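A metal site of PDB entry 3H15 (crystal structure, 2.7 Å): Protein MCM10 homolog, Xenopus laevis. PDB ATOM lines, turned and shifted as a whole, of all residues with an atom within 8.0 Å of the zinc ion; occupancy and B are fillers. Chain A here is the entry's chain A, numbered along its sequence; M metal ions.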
ATOM      1  N   THR A 151      -1.251  28.644 -17.478  1.00  0.00           N
ATOM      2  CA  THR A 151      -1.462  27.915 -18.729  1.00  0.00           C
ATOM      3  C   THR A 151      -2.843  27.274 -18.784  1.00  0.00           C
ATOM      4  O   THR A 151      -3.355  26.807 -17.764  1.00  0.00           O
ATOM      5  CB  THR A 151      -0.399  26.826 -18.905  1.00  0.00           C
ATOM      6  OG1 THR A 151       0.748  27.371 -19.558  1.00  0.00           O
ATOM      7  CG2 THR A 151      -0.943  25.670 -19.744  1.00  0.00           C
ATOM      8  N   CYS A 152      -3.432  27.237 -19.978  1.00  0.00           N
ATOM      9  CA  CYS A 152      -4.694  26.542 -20.168  1.00  0.00           C
ATOM     10  C   CYS A 152      -4.638  25.162 -19.522  1.00  0.00           C
ATOM     11  O   CYS A 152      -3.692  24.397 -19.754  1.00  0.00           O
ATOM     12  CB  CYS A 152      -5.044  26.420 -21.653  1.00  0.00           C
ATOM     13  SG  CYS A 152      -6.664  25.705 -21.962  1.00  0.00           S
ATOM     14  N   LYS A 153      -5.646  24.844 -18.726  1.00  0.00           N
ATOM     15  CA  LYS A 153      -5.701  23.597 -17.972  1.00  0.00           C
ATOM     16  C   LYS A 153      -6.139  22.415 -18.845  1.00  0.00           C
ATOM     17  O   LYS A 153      -6.017  21.257 -18.437  1.00  0.00           O
ATOM     18  CB  LYS A 153      -6.657  23.759 -16.772  1.00  0.00           C
ATOM     19  CG  LYS A 153      -6.792  22.535 -15.896  1.00  0.00           C
ATOM     20  CD  LYS A 153      -7.852  22.745 -14.825  1.00  0.00           C
ATOM     21  CE  LYS A 153      -7.817  21.641 -13.769  1.00  0.00           C
ATOM     22  NZ  LYS A 153      -8.108  20.294 -14.330  1.00  0.00           N
ATOM     23  N   ALA A 154      -6.638  22.716 -20.035  1.00  0.00           N
ATOM     24  CA  ALA A 154      -7.117  21.675 -20.952  1.00  0.00           C
ATOM     25  C   ALA A 154      -5.990  20.871 -21.582  1.00  0.00           C
ATOM     26  O   ALA A 154      -4.804  21.109 -21.331  1.00  0.00           O
ATOM     27  CB  ALA A 154      -8.004  22.289 -22.022  1.00  0.00           C
ATOM     28  N   ARG A 155      -6.379  19.896 -22.408  1.00  0.00           N
ATOM     29  CA  ARG A 155      -5.438  19.059 -23.141  1.00  0.00           C
ATOM     30  C   ARG A 155      -5.666  19.114 -24.654  1.00  0.00           C
ATOM     31  O   ARG A 155      -6.806  18.976 -25.117  1.00  0.00           O
ATOM     32  CB  ARG A 155      -5.538  17.614 -22.657  1.00  0.00           C
ATOM     33  CG  ARG A 155      -4.340  17.150 -21.870  1.00  0.00           C
ATOM     34  CD  ARG A 155      -4.727  16.127 -20.819  1.00  0.00           C
ATOM     35  NE  ARG A 155      -3.631  15.212 -20.529  1.00  0.00           N
ATOM     36  CZ  ARG A 155      -2.433  15.585 -20.087  1.00  0.00           C
ATOM     37  NH1 ARG A 155      -1.500  14.677 -19.843  1.00  0.00           N
ATOM     38  NH2 ARG A 155      -2.168  16.879 -19.907  1.00  0.00           N
ATOM     39  N   LYS A 156      -4.584  19.313 -25.412  1.00  0.00           N
ATOM     40  CA  LYS A 156      -4.655  19.407 -26.868  1.00  0.00           C
ATOM     41  C   LYS A 156      -5.339  18.181 -27.469  1.00  0.00           C
ATOM     42  O   LYS A 156      -4.713  17.128 -27.570  1.00  0.00           O
ATOM     43  CB  LYS A 156      -3.258  19.516 -27.469  1.00  0.00           C
ATOM     44  CG  LYS A 156      -2.665  20.909 -27.551  1.00  0.00           C
ATOM     45  CD  LYS A 156      -1.611  20.964 -28.663  1.00  0.00           C
ATOM     46  CE  LYS A 156      -0.308  21.598 -28.197  1.00  0.00           C
ATOM     47  NZ  LYS A 156       0.412  20.727 -27.213  1.00  0.00           N
ATOM     48  N   PRO A 161      -0.663  18.473 -23.219  1.00  0.00           N
ATOM     49  CA  PRO A 161      -1.467  19.457 -22.498  1.00  0.00           C
ATOM     50  C   PRO A 161      -1.452  20.762 -23.275  1.00  0.00           C
ATOM     51  O   PRO A 161      -0.458  21.057 -23.937  1.00  0.00           O
ATOM     52  CB  PRO A 161      -0.703  19.625 -21.183  1.00  0.00           C
ATOM     53  CG  PRO A 161       0.533  18.707 -21.292  1.00  0.00           C
ATOM     54  CD  PRO A 161       0.718  18.457 -22.740  1.00  0.00           C
ATOM     55  N   CYS A 162      -2.543  21.520 -23.223  1.00  0.00           N
ATOM     56  CA  CYS A 162      -2.559  22.805 -23.908  1.00  0.00           C
ATOM     57  C   CYS A 162      -1.482  23.726 -23.369  1.00  0.00           C
ATOM     58  O   CYS A 162      -1.159  23.704 -22.176  1.00  0.00           O
ATOM     59  CB  CYS A 162      -3.926  23.488 -23.831  1.00  0.00           C
ATOM     60  SG  CYS A 162      -3.880  25.119 -24.611  1.00  0.00           S
ATOM     61  N   THR A 163      -0.945  24.564 -24.241  1.00  0.00           N
ATOM     62  CA  THR A 163       0.186  25.425 -23.917  1.00  0.00           C
ATOM     63  C   THR A 163      -0.179  26.923 -23.971  1.00  0.00           C
ATOM     64  O   THR A 163       0.681  27.784 -23.872  1.00  0.00           O
ATOM     65  CB  THR A 163       1.359  25.143 -24.895  1.00  0.00           C
ATOM     66  OG1 THR A 163       2.601  25.507 -24.288  1.00  0.00           O
ATOM     67  CG2 THR A 163       1.169  25.897 -26.224  1.00  0.00           C
ATOM     68  N   GLN A 164      -1.466  27.217 -24.144  1.00  0.00           N
ATOM     69  CA  GLN A 164      -1.892  28.594 -24.349  1.00  0.00           C
ATOM     70  C   GLN A 164      -1.822  29.388 -23.055  1.00  0.00           C
ATOM     71  O   GLN A 164      -2.159  28.889 -21.986  1.00  0.00           O
ATOM     72  CB  GLN A 164      -3.319  28.618 -24.915  1.00  0.00           C
ATOM     73  CG  GLN A 164      -3.708  29.954 -25.510  1.00  0.00           C
ATOM     74  CD  GLN A 164      -3.375  30.048 -26.995  1.00  0.00           C
ATOM     75  OE1 GLN A 164      -3.235  29.025 -27.673  1.00  0.00           O
ATOM     76  NE2 GLN A 164      -3.259  31.272 -27.501  1.00  0.00           N
ATOM     77  N   MET A 165      -1.371  30.644 -23.150  1.00  0.00           N
ATOM     78  CA  MET A 165      -1.209  31.462 -21.953  1.00  0.00           C
ATOM     79  C   MET A 165      -2.539  31.943 -21.436  1.00  0.00           C
ATOM     80  O   MET A 165      -3.463  32.222 -22.203  1.00  0.00           O
ATOM     81  CB  MET A 165      -0.321  32.672 -22.221  1.00  0.00           C
ATOM     82  CG  MET A 165       0.004  33.445 -20.962  1.00  0.00           C
ATOM     83  SD  MET A 165       1.072  34.838 -21.300  1.00  0.00           S
ATOM     84  CE  MET A 165       2.461  34.012 -22.084  1.00  0.00           C
ATOM     85  N   VAL A 166      -2.643  32.068 -20.119  1.00  0.00           N
ATOM     86  CA  VAL A 166      -3.927  32.263 -19.476  1.00  0.00           C
ATOM     87  C   VAL A 166      -3.837  33.095 -18.211  1.00  0.00           C
ATOM     88  O   VAL A 166      -2.794  33.117 -17.546  1.00  0.00           O
ATOM     89  CB  VAL A 166      -4.563  30.893 -19.159  1.00  0.00           C
ATOM     90  CG1 VAL A 166      -5.213  30.899 -17.795  1.00  0.00           C
ATOM     91  CG2 VAL A 166      -5.547  30.493 -20.243  1.00  0.00           C
ATOM     92  N   GLU A 172      -9.497  29.846 -16.519  1.00  0.00           N
ATOM     93  CA  GLU A 172      -8.529  28.789 -16.288  1.00  0.00           C
ATOM     94  C   GLU A 172      -8.264  28.052 -17.589  1.00  0.00           C
ATOM     95  O   GLU A 172      -7.241  27.392 -17.749  1.00  0.00           O
ATOM     96  CB  GLU A 172      -9.095  27.824 -15.242  1.00  0.00           C
ATOM     97  CG  GLU A 172      -8.059  27.216 -14.313  1.00  0.00           C
ATOM     98  CD  GLU A 172      -8.705  26.487 -13.132  1.00  0.00           C
ATOM     99  OE1 GLU A 172      -9.922  26.184 -13.208  1.00  0.00           O
ATOM    100  OE2 GLU A 172      -7.991  26.207 -12.147  1.00  0.00           O
ATOM    101  N   TYR A 173      -9.197  28.177 -18.516  1.00  0.00           N
ATOM    102  CA  TYR A 173      -9.052  27.581 -19.819  1.00  0.00           C
ATOM    103  C   TYR A 173      -8.732  28.710 -20.767  1.00  0.00           C
ATOM    104  O   TYR A 173      -8.973  29.876 -20.436  1.00  0.00           O
ATOM    105  CB  TYR A 173     -10.356  26.896 -20.252  1.00  0.00           C
ATOM    106  CG  TYR A 173     -10.967  25.988 -19.212  1.00  0.00           C
ATOM    107  CD1 TYR A 173     -12.005  26.430 -18.404  1.00  0.00           C
ATOM    108  CD2 TYR A 173     -10.512  24.684 -19.032  1.00  0.00           C
ATOM    109  CE1 TYR A 173     -12.574  25.602 -17.451  1.00  0.00           C
ATOM    110  CE2 TYR A 173     -11.067  23.856 -18.075  1.00  0.00           C
ATOM    111  CZ  TYR A 173     -12.096  24.315 -17.293  1.00  0.00           C
ATOM    112  OH  TYR A 173     -12.654  23.491 -16.349  1.00  0.00           O
ATOM    113  N   CYS A 174      -8.190  28.387 -21.928  1.00  0.00           N
ATOM    114  CA  CYS A 174      -7.882  29.396 -22.920  1.00  0.00           C
ATOM    115  C   CYS A 174      -9.065  29.658 -23.837  1.00  0.00           C
ATOM    116  O   CYS A 174     -10.121  29.062 -23.685  1.00  0.00           O
ATOM    117  CB  CYS A 174      -6.686  28.966 -23.776  1.00  0.00           C
ATOM    118  SG  CYS A 174      -7.113  27.770 -25.046  1.00  0.00           S
ATOM    119  N   GLN A 175      -8.871  30.558 -24.785  1.00  0.00           N
ATOM    120  CA  GLN A 175      -9.919  30.982 -25.707  1.00  0.00           C
ATOM    121  C   GLN A 175     -10.470  29.817 -26.525  1.00  0.00           C
ATOM    122  O   GLN A 175     -11.657  29.760 -26.836  1.00  0.00           O
ATOM    123  CB  GLN A 175      -9.361  32.032 -26.655  1.00  0.00           C
ATOM    124  CG  GLN A 175     -10.030  32.114 -28.009  1.00  0.00           C
ATOM    125  CD  GLN A 175      -9.189  32.898 -28.986  1.00  0.00           C
ATOM    126  OE1 GLN A 175      -8.176  33.477 -28.607  1.00  0.00           O
ATOM    127  NE2 GLN A 175      -9.596  32.914 -30.248  1.00  0.00           N
ATOM    128  N   TYR A 176      -9.582  28.890 -26.854  1.00  0.00           N
ATOM    129  CA  TYR A 176      -9.923  27.810 -27.771  1.00  0.00           C
ATOM    130  C   TYR A 176     -10.465  26.569 -27.074  1.00  0.00           C
ATOM    131  O   TYR A 176     -10.545  25.509 -27.678  1.00  0.00           O
ATOM    132  CB  TYR A 176      -8.671  27.442 -28.576  1.00  0.00           C
ATOM    133  CG  TYR A 176      -8.078  28.587 -29.370  1.00  0.00           C
ATOM    134  CD1 TYR A 176      -6.874  29.167 -28.979  1.00  0.00           C
ATOM    135  CD2 TYR A 176      -8.712  29.083 -30.498  1.00  0.00           C
ATOM    136  CE1 TYR A 176      -6.318  30.216 -29.709  1.00  0.00           C
ATOM    137  CE2 TYR A 176      -8.164  30.136 -31.224  1.00  0.00           C
ATOM    138  CZ  TYR A 176      -6.972  30.689 -30.826  1.00  0.00           C
ATOM    139  OH  TYR A 176      -6.437  31.727 -31.563  1.00  0.00           O
ATOM    140  N   HIS A 177     -10.831  26.696 -25.797  1.00  0.00           N
ATOM    141  CA  HIS A 177     -11.377  25.586 -25.024  1.00  0.00           C
ATOM    142  C   HIS A 177     -12.428  26.104 -24.034  1.00  0.00           C
ATOM    143  O   HIS A 177     -12.074  26.553 -22.942  1.00  0.00           O
ATOM    144  CB  HIS A 177     -10.278  24.834 -24.243  1.00  0.00           C
ATOM    145  CG  HIS A 177      -9.245  24.158 -25.104  1.00  0.00           C
ATOM    146  ND1 HIS A 177      -7.954  23.939 -24.685  1.00  0.00           N
ATOM    147  CD2 HIS A 177      -9.319  23.632 -26.353  1.00  0.00           C
ATOM    148  CE1 HIS A 177      -7.274  23.319 -25.638  1.00  0.00           C
ATOM    149  NE2 HIS A 177      -8.080  23.124 -26.658  1.00  0.00           N
ATOM    150  N   VAL A 178     -13.701  26.048 -24.404  1.00  0.00           N
ATOM    151  CA  VAL A 178     -14.735  26.614 -23.547  1.00  0.00           C
ATOM    152  C   VAL A 178     -16.026  25.783 -23.496  1.00  0.00           C
ATOM    153  O   VAL A 178     -16.336  25.029 -24.416  1.00  0.00           O
ATOM    154  CB  VAL A 178     -15.066  28.069 -23.937  1.00  0.00           C
ATOM    155  CG1 VAL A 178     -13.859  28.981 -23.672  1.00  0.00           C
ATOM    156  CG2 VAL A 178     -15.486  28.135 -25.401  1.00  0.00           C
HETATM  157 ZN    ZN M   1      -6.208  25.635 -24.341  1.00  0.00          ZN
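The backbone carbonyl oxygen (O) of Gln 164 sits at hydrogen-bond distance from the backbone NH (N) of Cys 152 (2.9 Å).
N of Cys 162 sits at hydrogen-bond distance from O of Ala 154, at 3.0 Å.
N of Tyr 176 sits close to SG of Cys 174 (3.3 Å).
The side-chain sulfur (SG) of Cys 162 sits close to the backbone NH (N) of Gln 164, 3.2 Å away.
SG of Cys 152 sits close to N of Ala 154 (3.6 Å).
Of the 19 residues printed, 4 come within 4 Å of the zinc ion.
The zinc ion is bound by SG of Cys 162 (2.4 Å), SG of Cys 152 (2.4 Å), SG of Cys 174 (2.4 Å) and ND1 of His 177 (2.5 Å).
The zinc ion has four donor atoms within binding distance.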
